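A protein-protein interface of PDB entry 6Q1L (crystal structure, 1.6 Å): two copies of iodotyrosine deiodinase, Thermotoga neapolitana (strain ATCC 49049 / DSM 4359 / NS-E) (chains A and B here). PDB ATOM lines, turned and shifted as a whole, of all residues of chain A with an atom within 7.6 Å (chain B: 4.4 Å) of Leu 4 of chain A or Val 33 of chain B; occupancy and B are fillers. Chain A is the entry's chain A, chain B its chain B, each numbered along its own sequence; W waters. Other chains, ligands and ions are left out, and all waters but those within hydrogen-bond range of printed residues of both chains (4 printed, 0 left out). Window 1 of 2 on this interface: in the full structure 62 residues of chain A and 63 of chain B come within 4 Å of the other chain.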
ATOM      1  N   MET A   3     -30.937   6.472   6.446  1.00  0.00           N
ATOM      2  CA  MET A   3     -31.565   5.159   6.525  1.00  0.00           C
ATOM      3  C   MET A   3     -30.567   4.032   6.262  1.00  0.00           C
ATOM      4  O   MET A   3     -29.565   4.217   5.570  1.00  0.00           O
ATOM      5  CB  MET A   3     -32.710   5.022   5.509  1.00  0.00           C
ATOM      6  CG  MET A   3     -33.863   6.007   5.672  1.00  0.00           C
ATOM      7  SD  MET A   3     -34.705   5.884   7.270  1.00  0.00           S
ATOM      8  CE  MET A   3     -35.578   4.316   7.113  1.00  0.00           C
ATOM      9  N   LEU A   4     -30.876   2.832   6.756  1.00  0.00           N
ATOM     10  CA  LEU A   4     -30.015   1.703   6.446  1.00  0.00           C
ATOM     11  C   LEU A   4     -29.910   1.486   4.949  1.00  0.00           C
ATOM     12  O   LEU A   4     -28.861   1.077   4.457  1.00  0.00           O
ATOM     13  CB  LEU A   4     -30.545   0.432   7.102  1.00  0.00           C
ATOM     14  CG  LEU A   4     -29.689  -0.820   6.923  1.00  0.00           C
ATOM     15  CD1 LEU A   4     -28.373  -0.656   7.641  1.00  0.00           C
ATOM     16  CD2 LEU A   4     -30.467  -2.025   7.431  1.00  0.00           C
ATOM     17  N   TYR A   5     -30.986   1.745   4.213  1.00  0.00           N
ATOM     18  CA  TYR A   5     -30.937   1.585   2.769  1.00  0.00           C
ATOM     19  C   TYR A   5     -29.817   2.417   2.169  1.00  0.00           C
ATOM     20  O   TYR A   5     -29.108   1.961   1.270  1.00  0.00           O
ATOM     21  CB  TYR A   5     -32.265   1.977   2.128  1.00  0.00           C
ATOM     22  CG  TYR A   5     -32.209   1.898   0.618  1.00  0.00           C
ATOM     23  CD1 TYR A   5     -32.330   0.688  -0.044  1.00  0.00           C
ATOM     24  CD2 TYR A   5     -31.996   3.038  -0.144  1.00  0.00           C
ATOM     25  CE1 TYR A   5     -32.277   0.603  -1.410  1.00  0.00           C
ATOM     26  CE2 TYR A   5     -31.939   2.963  -1.533  1.00  0.00           C
ATOM     27  CZ  TYR A   5     -32.073   1.732  -2.154  1.00  0.00           C
ATOM     28  OH  TYR A   5     -32.011   1.612  -3.523  1.00  0.00           O
ATOM     29  N   ASP A   6     -29.633   3.642   2.667  1.00  0.00           N
ATOM     30  CA  ASP A   6     -28.597   4.517   2.113  1.00  0.00           C
ATOM     31  C   ASP A   6     -27.207   3.950   2.374  1.00  0.00           C
ATOM     32  O   ASP A   6     -26.321   4.026   1.517  1.00  0.00           O
ATOM     33  CB  ASP A   6     -28.731   5.915   2.723  1.00  0.00           C
ATOM     34  CG  ASP A   6     -30.029   6.589   2.340  1.00  0.00           C
ATOM     35  OD1 ASP A   6     -30.353   6.652   1.130  1.00  0.00           O
ATOM     36  OD2 ASP A   6     -30.735   7.060   3.254  1.00  0.00           O
ATOM     37  N   LEU A   7     -27.005   3.377   3.549  1.00  0.00           N
ATOM     38  CA  LEU A   7     -25.728   2.754   3.855  1.00  0.00           C
ATOM     39  C   LEU A   7     -25.485   1.557   2.947  1.00  0.00           C
ATOM     40  O   LEU A   7     -24.404   1.395   2.368  1.00  0.00           O
ATOM     41  CB  LEU A   7     -25.741   2.335   5.325  1.00  0.00           C
ATOM     42  CG  LEU A   7     -24.424   1.792   5.848  1.00  0.00           C
ATOM     43  CD1 LEU A   7     -23.448   2.972   5.969  1.00  0.00           C
ATOM     44  CD2 LEU A   7     -24.678   1.116   7.178  1.00  0.00           C
ATOM     45  N   ALA A   8     -26.517   0.736   2.769  1.00  0.00           N
ATOM     46  CA  ALA A   8     -26.377  -0.445   1.947  1.00  0.00           C
ATOM     47  C   ALA A   8     -26.198  -0.068   0.487  1.00  0.00           C
ATOM     48  O   ALA A   8     -25.425  -0.708  -0.234  1.00  0.00           O
ATOM     49  CB  ALA A   8     -27.596  -1.343   2.126  1.00  0.00           C
ATOM     50  N   LYS A   9     -26.931   0.954   0.032  1.00  0.00           N
ATOM     51  CA  LYS A   9     -26.830   1.367  -1.363  1.00  0.00           C
ATOM     52  C   LYS A   9     -25.442   1.902  -1.665  1.00  0.00           C
ATOM     53  O   LYS A   9     -24.865   1.602  -2.726  1.00  0.00           O
ATOM     54  CB  LYS A   9     -27.879   2.426  -1.687  1.00  0.00           C
ATOM     55  CG  LYS A   9     -27.756   2.922  -3.119  1.00  0.00           C
ATOM     56  CD  LYS A   9     -29.037   3.544  -3.622  1.00  0.00           C
ATOM     57  CE  LYS A   9     -28.869   4.021  -5.070  1.00  0.00           C
ATOM     58  NZ  LYS A   9     -28.410   2.933  -5.998  1.00  0.00           N
ATOM     59  N   LYS A  10     -24.902   2.694  -0.739  1.00  0.00           N
ATOM     60  CA  LYS A  10     -23.595   3.323  -0.900  1.00  0.00           C
ATOM     61  C   LYS A  10     -22.476   2.302  -0.884  1.00  0.00           C
ATOM     62  O   LYS A  10     -21.474   2.468  -1.582  1.00  0.00           O
ATOM     63  CB  LYS A  10     -23.393   4.348   0.220  1.00  0.00           C
ATOM     64  CG  LYS A  10     -22.167   5.239   0.097  1.00  0.00           C
ATOM     65  CD  LYS A  10     -22.333   6.503   0.957  1.00  0.00           C
ATOM     66  CE  LYS A  10     -22.769   6.188   2.401  1.00  0.00           C
ATOM     67  NZ  LYS A  10     -21.683   5.631   3.275  1.00  0.00           N
ATOM     68  N   LEU A 126     -21.521  -3.770   6.526  1.00  0.00           N
ATOM     69  CA  LEU A 126     -22.233  -2.520   6.766  1.00  0.00           C
ATOM     70  C   LEU A 126     -21.507  -1.695   7.812  1.00  0.00           C
ATOM     71  O   LEU A 126     -21.412  -0.475   7.700  1.00  0.00           O
ATOM     72  CB  LEU A 126     -23.681  -2.814   7.159  1.00  0.00           C
ATOM     73  CG  LEU A 126     -24.557  -3.301   6.014  1.00  0.00           C
ATOM     74  CD1 LEU A 126     -25.865  -3.870   6.550  1.00  0.00           C
ATOM     75  CD2 LEU A 126     -24.816  -2.206   5.029  1.00  0.00           C
ATOM     76  N   LYS A 173     -19.959   1.202  -7.966  1.00  0.00           N
ATOM     77  CA  LYS A 173     -20.802   0.055  -7.677  1.00  0.00           C
ATOM     78  C   LYS A 173     -21.436  -0.470  -8.955  1.00  0.00           C
ATOM     79  O   LYS A 173     -21.795   0.304  -9.844  1.00  0.00           O
ATOM     80  CB  LYS A 173     -21.879   0.437  -6.680  1.00  0.00           C
ATOM     81  CG  LYS A 173     -22.605  -0.777  -6.083  1.00  0.00           C
ATOM     82  CD  LYS A 173     -23.468  -0.339  -4.931  1.00  0.00           C
ATOM     83  CE  LYS A 173     -24.054  -1.581  -4.287  1.00  0.00           C
ATOM     84  NZ  LYS A 173     -24.824  -1.367  -3.070  1.00  0.00           N
ATOM     85  N   ARG A 176     -27.749  -3.001  -9.882  1.00  0.00           N
ATOM     86  CA  ARG A 176     -28.571  -3.978  -9.199  1.00  0.00           C
ATOM     87  C   ARG A 176     -29.861  -4.105  -9.978  1.00  0.00           C
ATOM     88  O   ARG A 176     -30.530  -3.105 -10.226  1.00  0.00           O
ATOM     89  CB  ARG A 176     -28.895  -3.582  -7.762  1.00  0.00           C
ATOM     90  CG  ARG A 176     -27.712  -3.622  -6.818  1.00  0.00           C
ATOM     91  CD  ARG A 176     -27.157  -4.999  -6.632  1.00  0.00           C
ATOM     92  NE  ARG A 176     -26.188  -5.064  -5.553  1.00  0.00           N
ATOM     93  CZ  ARG A 176     -24.906  -4.722  -5.673  1.00  0.00           C
ATOM     94  NH1 ARG A 176     -24.443  -4.256  -6.837  1.00  0.00           N
ATOM     95  NH2 ARG A 176     -24.085  -4.851  -4.644  1.00  0.00           N
ATOM     96  N   VAL A 179     -35.312  -6.073  -7.021  1.00  0.00           N
ATOM     97  CA  VAL A 179     -35.464  -7.264  -6.201  1.00  0.00           C
ATOM     98  C   VAL A 179     -36.646  -8.066  -6.725  1.00  0.00           C
ATOM     99  O   VAL A 179     -37.640  -7.513  -7.205  1.00  0.00           O
ATOM    100  CB  VAL A 179     -35.627  -6.866  -4.719  1.00  0.00           C
ATOM    101  CG1 VAL A 179     -37.003  -6.299  -4.478  1.00  0.00           C
ATOM    102  CG2 VAL A 179     -35.339  -8.043  -3.803  1.00  0.00           C
ATOM    103  N   LEU B   4     -25.139   1.798  13.747  1.00  0.00           N
ATOM    104  CA  LEU B   4     -25.403   0.432  13.318  1.00  0.00           C
ATOM    105  C   LEU B   4     -25.235  -0.553  14.472  1.00  0.00           C
ATOM    106  O   LEU B   4     -25.990  -1.528  14.579  1.00  0.00           O
ATOM    107  CB  LEU B   4     -24.471   0.072  12.176  1.00  0.00           C
ATOM    108  CG  LEU B   4     -24.678  -1.281  11.505  1.00  0.00           C
ATOM    109  CD1 LEU B   4     -25.974  -1.360  10.708  1.00  0.00           C
ATOM    110  CD2 LEU B   4     -23.492  -1.522  10.583  1.00  0.00           C
ATOM    111  N   TYR B  29     -39.196  -2.729   1.673  1.00  0.00           N
ATOM    112  CA  TYR B  29     -38.028  -1.934   2.044  1.00  0.00           C
ATOM    113  C   TYR B  29     -36.865  -2.828   2.461  1.00  0.00           C
ATOM    114  O   TYR B  29     -35.728  -2.643   2.013  1.00  0.00           O
ATOM    115  CB  TYR B  29     -38.375  -0.985   3.195  1.00  0.00           C
ATOM    116  CG  TYR B  29     -37.160  -0.327   3.804  1.00  0.00           C
ATOM    117  CD1 TYR B  29     -36.608   0.809   3.238  1.00  0.00           C
ATOM    118  CD2 TYR B  29     -36.548  -0.846   4.945  1.00  0.00           C
ATOM    119  CE1 TYR B  29     -35.501   1.413   3.786  1.00  0.00           C
ATOM    120  CE2 TYR B  29     -35.420  -0.241   5.499  1.00  0.00           C
ATOM    121  CZ  TYR B  29     -34.909   0.888   4.898  1.00  0.00           C
ATOM    122  OH  TYR B  29     -33.816   1.525   5.408  1.00  0.00           O
ATOM    123  N   SER B  30     -37.128  -3.813   3.316  1.00  0.00           N
ATOM    124  CA  SER B  30     -36.044  -4.648   3.812  1.00  0.00           C
ATOM    125  C   SER B  30     -35.477  -5.514   2.702  1.00  0.00           C
ATOM    126  O   SER B  30     -34.280  -5.802   2.700  1.00  0.00           O
ATOM    127  CB  SER B  30     -36.496  -5.514   5.001  1.00  0.00           C
ATOM    128  OG  SER B  30     -37.190  -6.696   4.638  1.00  0.00           O
ATOM    129  N   LEU B  31     -36.307  -5.884   1.715  1.00  0.00           N
ATOM    130  CA  LEU B  31     -35.809  -6.660   0.596  1.00  0.00           C
ATOM    131  C   LEU B  31     -34.968  -5.783  -0.319  1.00  0.00           C
ATOM    132  O   LEU B  31     -33.953  -6.240  -0.869  1.00  0.00           O
ATOM    133  CB  LEU B  31     -36.981  -7.250  -0.183  1.00  0.00           C
ATOM    134  CG  LEU B  31     -37.928  -8.158   0.583  1.00  0.00           C
ATOM    135  CD1 LEU B  31     -38.893  -8.830  -0.357  1.00  0.00           C
ATOM    136  CD2 LEU B  31     -37.177  -9.189   1.392  1.00  0.00           C
ATOM    137  N   LYS B  32     -35.328  -4.507  -0.414  1.00  0.00           N
ATOM    138  CA  LYS B  32     -34.543  -3.579  -1.219  1.00  0.00           C
ATOM    139  C   LYS B  32     -33.195  -3.316  -0.584  1.00  0.00           C
ATOM    140  O   LYS B  32     -32.184  -3.202  -1.291  1.00  0.00           O
ATOM    141  CB  LYS B  32     -35.304  -2.272  -1.426  1.00  0.00           C
ATOM    142  CG  LYS B  32     -36.500  -2.477  -2.295  1.00  0.00           C
ATOM    143  CD  LYS B  32     -37.200  -1.170  -2.603  1.00  0.00           C
ATOM    144  CE  LYS B  32     -38.237  -1.373  -3.689  1.00  0.00           C
ATOM    145  NZ  LYS B  32     -39.125  -0.184  -3.849  1.00  0.00           N
ATOM    146  N   VAL B  33     -33.158  -3.201   0.750  1.00  0.00           N
ATOM    147  CA  VAL B  33     -31.887  -3.137   1.447  1.00  0.00           C
ATOM    148  C   VAL B  33     -31.062  -4.376   1.118  1.00  0.00           C
ATOM    149  O   VAL B  33     -29.898  -4.284   0.737  1.00  0.00           O
ATOM    150  CB  VAL B  33     -32.090  -2.997   2.968  1.00  0.00           C
ATOM    151  CG1 VAL B  33     -30.747  -3.014   3.645  1.00  0.00           C
ATOM    152  CG2 VAL B  33     -32.837  -1.721   3.334  1.00  0.00           C
ATOM    153  N   ALA B  34     -31.652  -5.558   1.279  1.00  0.00           N
ATOM    154  CA  ALA B  34     -30.887  -6.775   1.095  1.00  0.00           C
ATOM    155  C   ALA B  34     -30.337  -6.848  -0.319  1.00  0.00           C
ATOM    156  O   ALA B  34     -29.218  -7.331  -0.522  1.00  0.00           O
ATOM    157  CB  ALA B  34     -31.767  -7.986   1.380  1.00  0.00           C
ATOM    158  N   ASN B  35     -31.116  -6.345  -1.278  1.00  0.00           N
ATOM    159  CA  ASN B  35     -30.767  -6.418  -2.690  1.00  0.00           C
ATOM    160  C   ASN B  35     -29.551  -5.568  -3.022  1.00  0.00           C
ATOM    161  O   ASN B  35     -28.934  -5.769  -4.072  1.00  0.00           O
ATOM    162  CB  ASN B  35     -31.985  -5.967  -3.496  1.00  0.00           C
ATOM    163  CG  ASN B  35     -31.848  -6.238  -4.952  1.00  0.00           C
ATOM    164  OD1 ASN B  35     -31.626  -7.373  -5.375  1.00  0.00           O
ATOM    165  ND2 ASN B  35     -31.984  -5.170  -5.776  1.00  0.00           N
ATOM    166  N   GLU B  36     -29.183  -4.648  -2.142  1.00  0.00           N
ATOM    167  CA  GLU B  36     -27.999  -3.821  -2.326  1.00  0.00           C
ATOM    168  C   GLU B  36     -26.742  -4.522  -1.862  1.00  0.00           C
ATOM    169  O   GLU B  36     -25.648  -3.984  -2.054  1.00  0.00           O
ATOM    170  CB  GLU B  36     -28.173  -2.494  -1.580  1.00  0.00           C
ATOM    171  CG  GLU B  36     -29.231  -1.622  -2.162  1.00  0.00           C
ATOM    172  CD  GLU B  36     -28.848  -1.127  -3.530  1.00  0.00           C
ATOM    173  OE1 GLU B  36     -27.636  -0.934  -3.763  1.00  0.00           O
ATOM    174  OE2 GLU B  36     -29.738  -0.947  -4.399  1.00  0.00           O
ATOM    175  N   ALA B  37     -26.894  -5.673  -1.215  1.00  0.00           N
ATOM    176  CA  ALA B  37     -25.751  -6.416  -0.721  1.00  0.00           C
ATOM    177  C   ALA B  37     -24.869  -6.855  -1.873  1.00  0.00           C
ATOM    178  O   ALA B  37     -25.344  -7.015  -3.032  1.00  0.00           O
ATOM    179  CB  ALA B  37     -26.193  -7.660   0.038  1.00  0.00           C
ATOM    180  N   TYR B 123     -28.238  -8.262   5.965  1.00  0.00           N
ATOM    181  CA  TYR B 123     -28.781  -6.957   5.675  1.00  0.00           C
ATOM    182  C   TYR B 123     -30.261  -6.907   5.984  1.00  0.00           C
ATOM    183  O   TYR B 123     -30.757  -5.940   6.555  1.00  0.00           O
ATOM    184  CB  TYR B 123     -28.574  -6.674   4.179  1.00  0.00           C
ATOM    185  CG  TYR B 123     -27.238  -6.151   3.725  1.00  0.00           C
ATOM    186  CD1 TYR B 123     -26.033  -6.638   4.194  1.00  0.00           C
ATOM    187  CD2 TYR B 123     -27.204  -5.165   2.739  1.00  0.00           C
ATOM    188  CE1 TYR B 123     -24.823  -6.138   3.744  1.00  0.00           C
ATOM    189  CE2 TYR B 123     -26.010  -4.684   2.261  1.00  0.00           C
ATOM    190  CZ  TYR B 123     -24.818  -5.166   2.775  1.00  0.00           C
ATOM    191  OH  TYR B 123     -23.629  -4.666   2.299  1.00  0.00           O
ATOM    192  N   LEU B 126     -31.295  -6.672   9.642  1.00  0.00           N
ATOM    193  CA  LEU B 126     -31.100  -5.335  10.210  1.00  0.00           C
ATOM    194  C   LEU B 126     -32.157  -4.370   9.688  1.00  0.00           C
ATOM    195  O   LEU B 126     -32.629  -3.486  10.415  1.00  0.00           O
ATOM    196  CB  LEU B 126     -29.712  -4.826   9.866  1.00  0.00           C
ATOM    197  CG  LEU B 126     -28.589  -5.567  10.555  1.00  0.00           C
ATOM    198  CD1 LEU B 126     -27.316  -5.248   9.853  1.00  0.00           C
ATOM    199  CD2 LEU B 126     -28.523  -5.185  12.033  1.00  0.00           C
ATOM    200  N   ALA B 127     -32.553  -4.531   8.428  1.00  0.00           N
ATOM    201  CA  ALA B 127     -33.571  -3.660   7.865  1.00  0.00           C
ATOM    202  C   ALA B 127     -34.918  -3.889   8.515  1.00  0.00           C
ATOM    203  O   ALA B 127     -35.650  -2.928   8.791  1.00  0.00           O
ATOM    204  CB  ALA B 127     -33.655  -3.889   6.357  1.00  0.00           C
ATOM    205  N   GLU B 130     -34.686  -2.077  11.822  1.00  0.00           N
ATOM    206  CA  GLU B 130     -34.893  -0.648  11.563  1.00  0.00           C
ATOM    207  C   GLU B 130     -36.369  -0.296  11.414  1.00  0.00           C
ATOM    208  O   GLU B 130     -36.815   0.766  11.870  1.00  0.00           O
ATOM    209  CB  GLU B 130     -34.142  -0.237  10.284  1.00  0.00           C
ATOM    210  CG  GLU B 130     -34.101   1.255  10.086  1.00  0.00           C
ATOM    211  CD  GLU B 130     -33.481   1.624   8.766  1.00  0.00           C
ATOM    212  OE1 GLU B 130     -33.610   0.821   7.821  1.00  0.00           O
ATOM    213  OE2 GLU B 130     -32.858   2.697   8.682  1.00  0.00           O
HETATM  214  O   HOH W   1     -24.892  -8.164  -5.635  1.00  0.00           O
HETATM  215  O   HOH W   2     -33.522   4.594  10.205  1.00  0.00           O
HETATM  216  O   HOH W   3     -24.041  -3.025   0.131  1.00  0.00           O
HETATM  217  O   HOH W   4     -27.739   0.123  -6.522  1.00  0.00           O
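NH2 of Arg 176 of chain A lies within hydrogen-bond range of O of Glu 36 of chain B (3.1 Å). The side-chain amino group (NZ) of Lys 173 of chain A lies within salt-bridge range of the side-chain carboxylate (OE1) of Glu 36 of chain B (2.9 Å). The backbone carbonyl oxygen (O) of Asn 35 of chain B sits at hydrogen-bond distance from the guanidinium group (NE) of Arg 176 of chain A (3.2 Å). The backbone NH of Leu 4 of chain A sits at hydrogen-bond distance from the side-chain hydroxyl of Tyr 29 of chain B, 3.5 Å away. The backbone NH (N) of Leu 4 of chain A sits at hydrogen-bond distance from the side-chain carboxylate (OE2) of Glu 130 of chain B, 2.8 Å away. The guanidinium group (NH2) of Arg 176 of chain A sits at hydrogen-bond distance from the backbone carbonyl oxygen (O) of Ala 37 of chain B. The side-chain hydroxyl (OH) of Tyr 29 of chain B lies within hydrogen-bond range of the backbone NH (N) of Tyr 5 of chain A, 3.1 Å away.
Water W2 bridges OE2 of Glu 130 of chain B and SD of Met 3 of chain A. Water W3 lies within hydrogen-bond range of O of Ala 8 of chain A (2.7 Å), OH of Tyr 123 of chain B (2.8 Å) and O of Glu 36 of chain B (2.9 Å). Water W1 bridges the backbone carbonyl oxygen (O) of Ala 37 of chain B (2.9 Å) and the guanidinium group (NE) of Arg 176 of chain A (3.4 Å). Water W4 lies within hydrogen-bond range of NZ of Lys 9 of chain A (2.9 Å) and OE1 of Glu 36 of chain B (3.0 Å).
Printed residues of chain B within 4 Å of Leu 4 of chain A: Leu 4, Tyr 29, Val 33, Leu 126, Ala 127 and Glu 130. Of the printed residues of chain B, Lys 9 of chain A touches Glu 36. Printed residues of chain B within 4 Å of Lys 173 of chain A: Glu 36 (2.9 Å). Of chain A, only Leu 4 (3.9 Å), Tyr 5 (3.9 Å) and Ala 8 (3.9 Å) come within 4 Å of Val 33 of chain B. The nearest residue of chain B that does not touch Leu 4 of chain A is Tyr 123 of chain B (4.02 Å). The nearest residue of chain A that does not touch Val 33 of chain B is Leu 126 of chain A (5.7 Å). The nearest printed residue of chain A that does not touch Leu 4 of chain B is Leu 7 of chain A (4.5 Å).
Leu 4 of chain A touches its own counterpart, Leu 4 of chain B. Leu 4 of chain A touches Leu 126 of chain B, and with the chains exchanged Leu 126 of chain A touches Leu 4 of chain B. Leu 126 of chain A touches its own counterpart, Leu 126 of chain B. Positions printed for both chains: 4 and 126. Of the 25 pairs that touch across the chains among the printed residues, 4 have their exchanged pair printed and touching as well.
Hydrophobic or aromatic side chains of chain B that line the printed part of chain A: Leu 4, Tyr 29, Val 33, Tyr 123, Leu 126 and Ala 127. Of the 12 printed residues of chain A, 9 touch a printed residue of chain B. Hydrophobic or aromatic side chains of chain A within 4 Å of the printed part of chain B: Met 3, Leu 4, Tyr 5, Ala 8, Leu 126 and Val 179. Among the printed residues, 25 pairs touch across the chains. Among the printed residues, Asp or Glu carboxylates within 4 Å of a Lys or Arg side-chain nitrogen of the other chain: Lys 173 of chain A with Glu 36 of chain B (2.9 Å).
Among the printed residues, merely in contact across the chains: Met 3 of chain A with Tyr 29 of chain B (3.7 Å), Met 3 of chain A with Glu 130 of chain B (3.5 Å), Leu 4 of chain A with Leu 4 of chain B (3.96 Å), Leu 4 of chain A with Val 33 of chain B (3.9 Å), Leu 4 of chain A with Leu 126 of chain B (3.7 Å), Leu 4 of chain A with Ala 127 of chain B (3.4 Å), Tyr 5 of chain A with Lys 32 of chain B (3.8 Å), Tyr 5 of chain A with Val 33 of chain B (3.9 Å), Tyr 5 of chain A with Glu 36 of chain B (3.5 Å), Ala 8 of chain A with Val 33 of chain B (3.9 Å), Ala 8 of chain A with Glu 36 of chain B (3.5 Å), Ala 8 of chain A with Tyr 123 of chain B (3.7 Å), Lys 9 of chain A with Glu 36 of chain B (3.4 Å), Leu 126 of chain A with Leu 4 of chain B (3.4 Å), Leu 126 of chain A with Tyr 123 of chain B (3.6 Å), Leu 126 of chain A with Leu 126 of chain B (3.9 Å), Val 179 of chain A with Leu 31 of chain B (3.7 Å) and Val 179 of chain A with Asn 35 of chain B (3.7 Å).
The side-chain hydroxyl of Tyr 29 of chain B is in hydrogen-bond range of the side-chain carboxylate of Glu 130 of chain B, 2.5 Å away. N of Met 3 of chain A sits at hydrogen-bond distance from OD2 of Asp 6 of chain A, 3.3 Å away. O of Ala 8 of chain A sits at hydrogen-bond distance from NZ of Lys 173 of chain A (3.0 Å). O of Lys 9 of chain A lies within hydrogen-bond range of NZ of Lys 173 of chain A.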
